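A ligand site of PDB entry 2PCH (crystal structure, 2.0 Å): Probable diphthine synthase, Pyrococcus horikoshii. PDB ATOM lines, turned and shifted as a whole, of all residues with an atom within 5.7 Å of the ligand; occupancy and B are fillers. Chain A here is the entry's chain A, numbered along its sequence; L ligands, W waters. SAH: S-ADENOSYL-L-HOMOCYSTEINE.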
ATOM      1  N   LEU A  10       5.269  -1.009 -15.432  1.00  0.00           N
ATOM      2  CA  LEU A  10       4.645  -0.454 -16.627  1.00  0.00           C
ATOM      3  C   LEU A  10       3.438  -1.254 -17.150  1.00  0.00           C
ATOM      4  O   LEU A  10       2.363  -0.715 -17.364  1.00  0.00           O
ATOM      5  CB  LEU A  10       5.700  -0.373 -17.742  1.00  0.00           C
ATOM      6  CG  LEU A  10       6.781   0.674 -17.487  1.00  0.00           C
ATOM      7  CD1 LEU A  10       8.004   0.445 -18.381  1.00  0.00           C
ATOM      8  CD2 LEU A  10       6.313   2.099 -17.768  1.00  0.00           C
ATOM      9  N   TYR A  11       3.661  -2.560 -17.404  1.00  0.00           N
ATOM     10  CA  TYR A  11       2.722  -3.352 -18.221  1.00  0.00           C
ATOM     11  C   TYR A  11       2.051  -4.495 -17.437  1.00  0.00           C
ATOM     12  O   TYR A  11       0.840  -4.629 -17.403  1.00  0.00           O
ATOM     13  CB  TYR A  11       3.485  -3.921 -19.422  1.00  0.00           C
ATOM     14  CG  TYR A  11       2.519  -4.588 -20.341  1.00  0.00           C
ATOM     15  CD1 TYR A  11       1.468  -3.853 -20.904  1.00  0.00           C
ATOM     16  CD2 TYR A  11       2.687  -5.930 -20.682  1.00  0.00           C
ATOM     17  CE1 TYR A  11       0.605  -4.468 -21.803  1.00  0.00           C
ATOM     18  CE2 TYR A  11       1.812  -6.535 -21.574  1.00  0.00           C
ATOM     19  CZ  TYR A  11       0.772  -5.819 -22.132  1.00  0.00           C
ATOM     20  OH  TYR A  11      -0.082  -6.414 -23.032  1.00  0.00           O
ATOM     21  N   THR A  36      -4.852   5.306 -11.221  1.00  0.00           N
ATOM     22  CA  THR A  36      -3.893   6.315 -11.675  1.00  0.00           C
ATOM     23  C   THR A  36      -3.281   5.966 -13.022  1.00  0.00           C
ATOM     24  O   THR A  36      -2.770   6.836 -13.725  1.00  0.00           O
ATOM     25  CB  THR A  36      -2.760   6.534 -10.640  1.00  0.00           C
ATOM     26  OG1 THR A  36      -2.103   5.283 -10.371  1.00  0.00           O
ATOM     27  CG2 THR A  36      -3.324   7.101  -9.345  1.00  0.00           C
ATOM     28  N   SER A  37      -3.319   4.687 -13.383  1.00  0.00           N
ATOM     29  CA  SER A  37      -2.761   4.255 -14.656  1.00  0.00           C
ATOM     30  C   SER A  37      -3.328   2.904 -15.033  1.00  0.00           C
ATOM     31  O   SER A  37      -3.999   2.261 -14.222  1.00  0.00           O
ATOM     32  CB  SER A  37      -1.233   4.176 -14.570  1.00  0.00           C
ATOM     33  OG  SER A  37      -0.674   3.807 -15.820  1.00  0.00           O
ATOM     34  N   LEU A  38      -3.051   2.468 -16.260  1.00  0.00           N
ATOM     35  CA  LEU A  38      -3.549   1.181 -16.726  1.00  0.00           C
ATOM     36  C   LEU A  38      -2.429   0.181 -16.996  1.00  0.00           C
ATOM     37  O   LEU A  38      -1.531   0.438 -17.792  1.00  0.00           O
ATOM     38  CB  LEU A  38      -4.358   1.374 -18.017  1.00  0.00           C
ATOM     39  CG  LEU A  38      -4.847   0.081 -18.675  1.00  0.00           C
ATOM     40  CD1 LEU A  38      -5.892  -0.590 -17.798  1.00  0.00           C
ATOM     41  CD2 LEU A  38      -5.441   0.390 -20.048  1.00  0.00           C
ATOM     42  N   PRO A  85       0.277   1.244 -10.021  1.00  0.00           N
ATOM     43  CA  PRO A  85       0.868   0.950 -11.327  1.00  0.00           C
ATOM     44  C   PRO A  85       2.081   1.870 -11.463  1.00  0.00           C
ATOM     45  O   PRO A  85       2.202   2.845 -10.721  1.00  0.00           O
ATOM     46  CB  PRO A  85      -0.250   1.338 -12.306  1.00  0.00           C
ATOM     47  CG  PRO A  85      -1.521   1.210 -11.475  1.00  0.00           C
ATOM     48  CD  PRO A  85      -1.094   1.773 -10.150  1.00  0.00           C
ATOM     49  N   GLY A  86       2.982   1.552 -12.388  1.00  0.00           N
ATOM     50  CA  GLY A  86       4.174   2.371 -12.585  1.00  0.00           C
ATOM     51  C   GLY A  86       4.906   2.649 -11.286  1.00  0.00           C
ATOM     52  O   GLY A  86       5.067   1.766 -10.451  1.00  0.00           O
ATOM     53  N   ASP A  87       5.385   3.881 -11.123  1.00  0.00           N
ATOM     54  CA  ASP A  87       6.076   4.296  -9.909  1.00  0.00           C
ATOM     55  C   ASP A  87       4.992   5.010  -9.096  1.00  0.00           C
ATOM     56  O   ASP A  87       4.289   5.867  -9.618  1.00  0.00           O
ATOM     57  CB  ASP A  87       7.226   5.244 -10.242  1.00  0.00           C
ATOM     58  CG  ASP A  87       7.979   5.709  -8.995  1.00  0.00           C
ATOM     59  OD1 ASP A  87       7.398   6.479  -8.188  1.00  0.00           O
ATOM     60  OD2 ASP A  87       9.150   5.311  -8.834  1.00  0.00           O
ATOM     61  N   PRO A  88       4.863   4.655  -7.814  1.00  0.00           N
ATOM     62  CA  PRO A  88       3.841   5.252  -6.935  1.00  0.00           C
ATOM     63  C   PRO A  88       3.814   6.772  -6.768  1.00  0.00           C
ATOM     64  O   PRO A  88       2.757   7.338  -6.442  1.00  0.00           O
ATOM     65  CB  PRO A  88       4.075   4.525  -5.608  1.00  0.00           C
ATOM     66  CG  PRO A  88       5.546   4.245  -5.627  1.00  0.00           C
ATOM     67  CD  PRO A  88       5.774   3.787  -7.053  1.00  0.00           C
ATOM     68  N   LEU A  89       4.944   7.430  -6.996  1.00  0.00           N
ATOM     69  CA  LEU A  89       5.003   8.869  -6.805  1.00  0.00           C
ATOM     70  C   LEU A  89       5.167   9.694  -8.070  1.00  0.00           C
ATOM     71  O   LEU A  89       5.512  10.873  -8.002  1.00  0.00           O
ATOM     72  CB  LEU A  89       6.146   9.209  -5.845  1.00  0.00           C
ATOM     73  CG  LEU A  89       6.156   8.468  -4.501  1.00  0.00           C
ATOM     74  CD1 LEU A  89       7.285   9.025  -3.653  1.00  0.00           C
ATOM     75  CD2 LEU A  89       4.824   8.634  -3.790  1.00  0.00           C
ATOM     76  N   VAL A  90       4.910   9.088  -9.218  1.00  0.00           N
ATOM     77  CA  VAL A  90       5.038   9.786 -10.503  1.00  0.00           C
ATOM     78  C   VAL A  90       3.676  10.108 -11.104  1.00  0.00           C
ATOM     79  O   VAL A  90       2.877   9.203 -11.363  1.00  0.00           O
ATOM     80  CB  VAL A  90       5.830   8.941 -11.521  1.00  0.00           C
ATOM     81  CG1 VAL A  90       5.810   9.608 -12.877  1.00  0.00           C
ATOM     82  CG2 VAL A  90       7.258   8.749 -11.038  1.00  0.00           C
ATOM     83  N   ALA A  91       3.419  11.382 -11.342  1.00  0.00           N
ATOM     84  CA  ALA A  91       2.149  11.802 -11.940  1.00  0.00           C
ATOM     85  C   ALA A  91       0.943  11.333 -11.126  1.00  0.00           C
ATOM     86  O   ALA A  91      -0.084  10.956 -11.685  1.00  0.00           O
ATOM     87  CB  ALA A  91       2.049  11.297 -13.383  1.00  0.00           C
ATOM     88  N   THR A  92       1.100  11.337  -9.814  1.00  0.00           N
ATOM     89  CA  THR A  92       0.030  10.975  -8.890  1.00  0.00           C
ATOM     90  C   THR A  92       0.162  11.983  -7.773  1.00  0.00           C
ATOM     91  O   THR A  92       1.080  12.818  -7.782  1.00  0.00           O
ATOM     92  CB  THR A  92       0.214   9.574  -8.291  1.00  0.00           C
ATOM     93  OG1 THR A  92       1.337   9.590  -7.394  1.00  0.00           O
ATOM     94  CG2 THR A  92       0.435   8.545  -9.378  1.00  0.00           C
ATOM     95  N   PRO A 114       9.591   0.603 -12.780  1.00  0.00           N
ATOM     96  CA  PRO A 114       9.689   1.364 -14.037  1.00  0.00           C
ATOM     97  C   PRO A 114       8.478   2.268 -14.250  1.00  0.00           C
ATOM     98  O   PRO A 114       7.342   1.874 -14.016  1.00  0.00           O
ATOM     99  CB  PRO A 114       9.821   0.272 -15.100  1.00  0.00           C
ATOM    100  CG  PRO A 114      10.250  -0.995 -14.396  1.00  0.00           C
ATOM    101  CD  PRO A 114       9.654  -0.845 -13.031  1.00  0.00           C
ATOM    102  N   SER A 115       8.753   3.502 -14.691  1.00  0.00           N
ATOM    103  CA  SER A 115       7.717   4.508 -14.919  1.00  0.00           C
ATOM    104  C   SER A 115       7.681   4.958 -16.372  1.00  0.00           C
ATOM    105  O   SER A 115       8.700   4.955 -17.064  1.00  0.00           O
ATOM    106  CB  SER A 115       7.986   5.726 -14.032  1.00  0.00           C
ATOM    107  OG  SER A 115       7.168   6.818 -14.409  1.00  0.00           O
ATOM    108  N   ILE A 116       6.505   5.371 -16.853  1.00  0.00           N
ATOM    109  CA  ILE A 116       6.384   5.837 -18.220  1.00  0.00           C
ATOM    110  C   ILE A 116       7.271   7.070 -18.408  1.00  0.00           C
ATOM    111  O   ILE A 116       7.786   7.338 -19.503  1.00  0.00           O
ATOM    112  CB  ILE A 116       4.907   6.208 -18.560  1.00  0.00           C
ATOM    113  CG1 ILE A 116       4.776   6.534 -20.053  1.00  0.00           C
ATOM    114  CG2 ILE A 116       4.443   7.388 -17.706  1.00  0.00           C
ATOM    115  CD1 ILE A 116       5.047   5.351 -20.970  1.00  0.00           C
ATOM    116  N   TYR A 117       7.484   7.806 -17.325  1.00  0.00           N
ATOM    117  CA  TYR A 117       8.306   9.010 -17.397  1.00  0.00           C
ATOM    118  C   TYR A 117       9.729   8.720 -17.894  1.00  0.00           C
ATOM    119  O   TYR A 117      10.316   9.544 -18.599  1.00  0.00           O
ATOM    120  CB  TYR A 117       8.349   9.684 -16.017  1.00  0.00           C
ATOM    121  CG  TYR A 117       8.872  11.103 -16.064  1.00  0.00           C
ATOM    122  CD1 TYR A 117       8.108  12.132 -16.628  1.00  0.00           C
ATOM    123  CD2 TYR A 117      10.140  11.416 -15.581  1.00  0.00           C
ATOM    124  CE1 TYR A 117       8.608  13.432 -16.715  1.00  0.00           C
ATOM    125  CE2 TYR A 117      10.651  12.707 -15.665  1.00  0.00           C
ATOM    126  CZ  TYR A 117       9.889  13.707 -16.225  1.00  0.00           C
ATOM    127  OH  TYR A 117      10.403  14.977 -16.315  1.00  0.00           O
ATOM    128  N   LEU A 164       3.174  14.065 -22.965  1.00  0.00           N
ATOM    129  CA  LEU A 164       1.769  14.278 -22.670  1.00  0.00           C
ATOM    130  C   LEU A 164       1.116  13.020 -22.134  1.00  0.00           C
ATOM    131  O   LEU A 164       0.881  12.049 -22.864  1.00  0.00           O
ATOM    132  CB  LEU A 164       1.014  14.722 -23.934  1.00  0.00           C
ATOM    133  CG  LEU A 164       1.463  16.042 -24.573  1.00  0.00           C
ATOM    134  CD1 LEU A 164       0.800  16.205 -25.938  1.00  0.00           C
ATOM    135  CD2 LEU A 164       1.093  17.189 -23.648  1.00  0.00           C
ATOM    136  N   PHE A 165       0.838  13.012 -20.830  1.00  0.00           N
ATOM    137  CA  PHE A 165       0.160  11.895 -20.214  1.00  0.00           C
ATOM    138  C   PHE A 165      -1.254  12.038 -20.759  1.00  0.00           C
ATOM    139  O   PHE A 165      -1.724  13.159 -20.971  1.00  0.00           O
ATOM    140  CB  PHE A 165       0.129  12.056 -18.697  1.00  0.00           C
ATOM    141  CG  PHE A 165       1.478  11.995 -18.040  1.00  0.00           C
ATOM    142  CD1 PHE A 165       2.058  10.762 -17.745  1.00  0.00           C
ATOM    143  CD2 PHE A 165       2.149  13.156 -17.693  1.00  0.00           C
ATOM    144  CE1 PHE A 165       3.308  10.701 -17.104  1.00  0.00           C
ATOM    145  CE2 PHE A 165       3.398  13.105 -17.053  1.00  0.00           C
ATOM    146  CZ  PHE A 165       3.968  11.872 -16.760  1.00  0.00           C
ATOM    147  N   LEU A 166      -1.938  10.924 -20.982  1.00  0.00           N
ATOM    148  CA  LEU A 166      -3.298  10.984 -21.498  1.00  0.00           C
ATOM    149  C   LEU A 166      -4.289  10.655 -20.381  1.00  0.00           C
ATOM    150  O   LEU A 166      -3.996   9.872 -19.476  1.00  0.00           O
ATOM    151  CB  LEU A 166      -3.455  10.054 -22.701  1.00  0.00           C
ATOM    152  CG  LEU A 166      -2.465  10.319 -23.840  1.00  0.00           C
ATOM    153  CD1 LEU A 166      -2.853   9.500 -25.064  1.00  0.00           C
ATOM    154  CD2 LEU A 166      -2.470  11.808 -24.197  1.00  0.00           C
ATOM    155  N   ASP A 167      -5.472  11.247 -20.447  1.00  0.00           N
ATOM    156  CA  ASP A 167      -6.490  11.043 -19.432  1.00  0.00           C
ATOM    157  C   ASP A 167      -6.918   9.589 -19.253  1.00  0.00           C
ATOM    158  O   ASP A 167      -6.746   8.748 -20.137  1.00  0.00           O
ATOM    159  CB  ASP A 167      -7.723  11.892 -19.733  1.00  0.00           C
ATOM    160  CG  ASP A 167      -8.380  12.427 -18.480  1.00  0.00           C
ATOM    161  OD1 ASP A 167      -8.051  11.928 -17.381  1.00  0.00           O
ATOM    162  OD2 ASP A 167      -9.222  13.333 -18.581  1.00  0.00           O
ATOM    163  N   ILE A 168      -7.506   9.326 -18.089  1.00  0.00           N
ATOM    164  CA  ILE A 168      -7.990   8.001 -17.751  1.00  0.00           C
ATOM    165  C   ILE A 168      -9.146   8.108 -16.759  1.00  0.00           C
ATOM    166  O   ILE A 168      -9.090   8.867 -15.786  1.00  0.00           O
ATOM    167  CB  ILE A 168      -6.865   7.120 -17.117  1.00  0.00           C
ATOM    168  CG1 ILE A 168      -7.459   5.831 -16.546  1.00  0.00           C
ATOM    169  CG2 ILE A 168      -6.127   7.904 -16.035  1.00  0.00           C
ATOM    170  CD1 ILE A 168      -6.441   4.928 -15.865  1.00  0.00           C
ATOM    171  N   LEU A 206       3.693   6.257 -28.111  1.00  0.00           N
ATOM    172  CA  LEU A 206       4.228   5.088 -27.423  1.00  0.00           C
ATOM    173  C   LEU A 206       3.032   4.426 -26.756  1.00  0.00           C
ATOM    174  O   LEU A 206       2.368   5.035 -25.901  1.00  0.00           O
ATOM    175  CB  LEU A 206       5.259   5.504 -26.369  1.00  0.00           C
ATOM    176  CG  LEU A 206       5.880   4.371 -25.538  1.00  0.00           C
ATOM    177  CD1 LEU A 206       6.456   3.282 -26.448  1.00  0.00           C
ATOM    178  CD2 LEU A 206       6.958   4.953 -24.631  1.00  0.00           C
ATOM    179  N   ALA A 207       2.731   3.203 -27.158  1.00  0.00           N
ATOM    180  CA  ALA A 207       1.609   2.470 -26.603  1.00  0.00           C
ATOM    181  C   ALA A 207       2.041   1.166 -25.955  1.00  0.00           C
ATOM    182  O   ALA A 207       2.802   0.398 -26.548  1.00  0.00           O
ATOM    183  CB  ALA A 207       0.574   2.178 -27.704  1.00  0.00           C
ATOM    184  N   ARG A 208       1.553   0.948 -24.739  1.00  0.00           N
ATOM    185  CA  ARG A 208       1.847  -0.261 -23.983  1.00  0.00           C
ATOM    186  C   ARG A 208       3.334  -0.436 -23.698  1.00  0.00           C
ATOM    187  O   ARG A 208       3.904  -1.517 -23.904  1.00  0.00           O
ATOM    188  CB  ARG A 208       1.292  -1.479 -24.723  1.00  0.00           C
ATOM    189  CG  ARG A 208      -0.219  -1.395 -24.991  1.00  0.00           C
ATOM    190  CD  ARG A 208      -0.732  -2.649 -25.720  1.00  0.00           C
ATOM    191  NE  ARG A 208       0.034  -2.897 -26.941  1.00  0.00           N
ATOM    192  CZ  ARG A 208      -0.016  -2.133 -28.029  1.00  0.00           C
ATOM    193  NH1 ARG A 208      -0.810  -1.073 -28.071  1.00  0.00           N
ATOM    194  NH2 ARG A 208       0.740  -2.429 -29.083  1.00  0.00           N
ATOM    195  N   ALA A 209       3.964   0.630 -23.222  1.00  0.00           N
ATOM    196  CA  ALA A 209       5.367   0.590 -22.865  1.00  0.00           C
ATOM    197  C   ALA A 209       5.449  -0.498 -21.792  1.00  0.00           C
ATOM    198  O   ALA A 209       4.513  -0.657 -21.005  1.00  0.00           O
ATOM    199  CB  ALA A 209       5.790   1.940 -22.276  1.00  0.00           C
ATOM    200  N   GLY A 210       6.543  -1.245 -21.772  1.00  0.00           N
ATOM    201  CA  GLY A 210       6.664  -2.291 -20.779  1.00  0.00           C
ATOM    202  C   GLY A 210       6.394  -3.659 -21.361  1.00  0.00           C
ATOM    203  O   GLY A 210       6.937  -4.667 -20.897  1.00  0.00           O
ATOM    204  N   PRO A 233      -2.600   1.437 -22.498  1.00  0.00           N
ATOM    205  CA  PRO A 233      -2.468   2.898 -22.472  1.00  0.00           C
ATOM    206  C   PRO A 233      -1.545   3.451 -23.547  1.00  0.00           C
ATOM    207  O   PRO A 233      -0.696   2.739 -24.082  1.00  0.00           O
ATOM    208  CB  PRO A 233      -1.942   3.155 -21.071  1.00  0.00           C
ATOM    209  CG  PRO A 233      -1.000   2.015 -20.882  1.00  0.00           C
ATOM    210  CD  PRO A 233      -1.754   0.824 -21.464  1.00  0.00           C
ATOM    211  N   HIS A 234      -1.731   4.731 -23.855  1.00  0.00           N
ATOM    212  CA  HIS A 234      -0.926   5.419 -24.844  1.00  0.00           C
ATOM    213  C   HIS A 234      -0.442   6.718 -24.218  1.00  0.00           C
ATOM    214  O   HIS A 234      -1.066   7.237 -23.305  1.00  0.00           O
ATOM    215  CB  HIS A 234      -1.760   5.865 -26.060  1.00  0.00           C
ATOM    216  CG  HIS A 234      -2.390   4.747 -26.835  1.00  0.00           C
ATOM    217  ND1 HIS A 234      -3.193   4.990 -27.927  1.00  0.00           N
ATOM    218  CD2 HIS A 234      -2.313   3.404 -26.710  1.00  0.00           C
ATOM    219  CE1 HIS A 234      -3.585   3.835 -28.444  1.00  0.00           C
ATOM    220  NE2 HIS A 234      -3.063   2.862 -27.722  1.00  0.00           N
ATOM    221  N   ILE A 235       0.673   7.234 -24.726  1.00  0.00           N
ATOM    222  CA  ILE A 235       1.156   8.544 -24.306  1.00  0.00           C
ATOM    223  C   ILE A 235       1.505   9.204 -25.622  1.00  0.00           C
ATOM    224  O   ILE A 235       1.837   8.533 -26.594  1.00  0.00           O
ATOM    225  CB  ILE A 235       2.435   8.548 -23.434  1.00  0.00           C
ATOM    226  CG1 ILE A 235       3.613   7.949 -24.196  1.00  0.00           C
ATOM    227  CG2 ILE A 235       2.175   7.841 -22.139  1.00  0.00           C
ATOM    228  CD1 ILE A 235       4.941   8.266 -23.571  1.00  0.00           C
HETATM  229  N   SAH L   1       2.741   6.656 -11.831  1.00  0.00           N
HETATM  230  CA  SAH L   1       2.543   6.234 -13.280  1.00  0.00           C
HETATM  231  CB  SAH L   1       1.849   7.197 -14.202  1.00  0.00           C
HETATM  232  CG  SAH L   1       0.463   7.680 -13.868  1.00  0.00           C
HETATM  233  SD  SAH L   1      -0.093   8.680 -15.314  1.00  0.00           S
HETATM  234  C   SAH L   1       3.992   5.876 -13.845  1.00  0.00           C
HETATM  235  O   SAH L   1       4.974   5.994 -13.087  1.00  0.00           O
HETATM  236  OXT SAH L   1       4.046   5.471 -15.091  1.00  0.00           O
HETATM  237  C5' SAH L   1      -0.980   7.475 -16.222  1.00  0.00           C
HETATM  238  C4' SAH L   1      -0.861   7.813 -17.758  1.00  0.00           C
HETATM  239  O4' SAH L   1       0.515   7.616 -18.141  1.00  0.00           O
HETATM  240  C3' SAH L   1      -1.679   6.956 -18.670  1.00  0.00           C
HETATM  241  O3' SAH L   1      -2.977   7.517 -18.831  1.00  0.00           O
HETATM  242  C2' SAH L   1      -0.823   6.929 -19.946  1.00  0.00           C
HETATM  243  O2' SAH L   1      -1.070   8.080 -20.779  1.00  0.00           O
HETATM  244  C1' SAH L   1       0.619   6.845 -19.424  1.00  0.00           C
HETATM  245  N9  SAH L   1       1.072   5.583 -19.207  1.00  0.00           N
HETATM  246  C8  SAH L   1       1.261   4.793 -18.083  1.00  0.00           C
HETATM  247  N7  SAH L   1       1.734   3.609 -18.323  1.00  0.00           N
HETATM  248  C5  SAH L   1       1.890   3.563 -19.732  1.00  0.00           C
HETATM  249  C6  SAH L   1       2.375   2.523 -20.611  1.00  0.00           C
HETATM  250  N6  SAH L   1       2.799   1.328 -20.183  1.00  0.00           N
HETATM  251  N1  SAH L   1       2.384   2.851 -21.949  1.00  0.00           N
HETATM  252  C2  SAH L   1       1.976   4.059 -22.427  1.00  0.00           C
HETATM  253  N3  SAH L   1       1.505   5.070 -21.624  1.00  0.00           N
HETATM  254  C4  SAH L   1       1.496   4.752 -20.287  1.00  0.00           C
HETATM  255  O   HOH W   1       2.437   2.779 -15.394  1.00  0.00           O
HETATM  256  O   HOH W   2      -5.291   6.325 -20.046  1.00  0.00           O
HETATM  257  O   HOH W   3      -3.344  10.234 -16.822  1.00  0.00           O
HETATM  258  O   HOH W   4       0.379   5.136 -10.978  1.00  0.00           O
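The backbone carbonyl oxygen of Val 90 is in hydrogen-bond range of a nitrogen (N) of the ligand (2.6 Å).
The backbone NH (N) of Leu 166 is in hydrogen-bond range of an oxygen (O2') of the ligand (3.0 Å).
O of Leu 166 is in hydrogen-bond range of O3' of the ligand (2.6 Å).
The backbone carbonyl oxygen (O) of His 234 lies within hydrogen-bond range of an oxygen (O2') of the ligand, 2.7 Å away.
An oxygen (O) of the ligand sits at hydrogen-bond distance from the side-chain hydroxyl (OG) of Ser 115 (2.7 Å).
A nitrogen (N1) of the ligand sits at hydrogen-bond distance from the backbone NH (N) of Ala 209 (3.0 Å).
The backbone carbonyl oxygen (O) of Ala 209 lies within hydrogen-bond range of a nitrogen (N6) of the ligand, 2.7 Å away.
O of the ligand is in hydrogen-bond range of N of Asp 87.
A nitrogen (N) of the ligand is in hydrogen-bond range of the backbone carbonyl oxygen (O) of Asp 87 (2.8 Å).
N of Ile 116 sits at hydrogen-bond distance from OXT of the ligand (3.0 Å).
OG of Ser 37 sits close to N7 of the ligand (3.5 Å).
A nitrogen (N1) of the ligand sits at hydrogen-bond distance from the backbone NH of Arg 208 (3.5 Å).
N of Tyr 117 lies close to OG of Ser 115 (3.1 Å).
The side-chain carboxylate (OD1) of Asp 87 lies within hydrogen-bond range of the backbone NH (N) of Leu 89.
The backbone NH (N) of Ile 235 is in hydrogen-bond range of the backbone carbonyl oxygen (O) of Leu 206 (3.0 Å).
O of Pro 233 is in hydrogen-bond range of N of Arg 208, at 2.9 Å.
OG1 of Thr 92 is in hydrogen-bond range of O of Pro 88 (2.8 Å).
The backbone carbonyl oxygen of Thr 36 lies close to a sulfur (SD) of the ligand (3.6 Å).
O of Leu 10 touches N6 of the ligand, at 3.5 Å.
Gly 86 touches the ligand.
Ala 91 touches the ligand (CB to SD, 3.9 Å).
CG2 of Thr 92 touches N of the ligand (3.9 Å).
Phe 165 touches the ligand (CD1 to O4', 3.5 Å).
Leu 206 touches the ligand.
O of Pro 233 touches C2 of the ligand, at 3.4 Å.
Ile 235 touches the ligand.
Hydrophobic or aromatic side chains within 4 Å of the ligand: Val 90, Ala 91, Ile 116, Phe 165, Leu 166, Ala 209, Pro 233 and Ile 235.
Within 4 Å of the ligand: Leu 10, Thr 36, Ser 37, Gly 86, Asp 87, Val 90, Ala 91, Thr 92, Ser 115, Ile 116, Phe 165, Leu 166, Leu 206, Arg 208, Ala 209, Pro 233, His 234 and Ile 235.
The nearest printed residue that does not touch the ligand is Pro 85 (4.01 Å).
Water W2 lies within hydrogen-bond range of O of Asp 167 (2.8 Å) and O3' of the ligand (2.9 Å).
Water W4 lies within hydrogen-bond range of the side-chain hydroxyl (OG1) of Thr 36 (2.6 Å), a nitrogen (N) of the ligand (2.9 Å) and the backbone carbonyl oxygen (O) of Pro 85 (2.9 Å).
Water W1 lies within hydrogen-bond range of a nitrogen (N7) of the ligand, the backbone NH (N) of Gly 86 and the side-chain hydroxyl (OG) of Ser 37.
Water W3 lies within hydrogen-bond range of the backbone carbonyl oxygen of Leu 166 (2.8 Å) and an oxygen (O3') of the ligand (3.4 Å).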
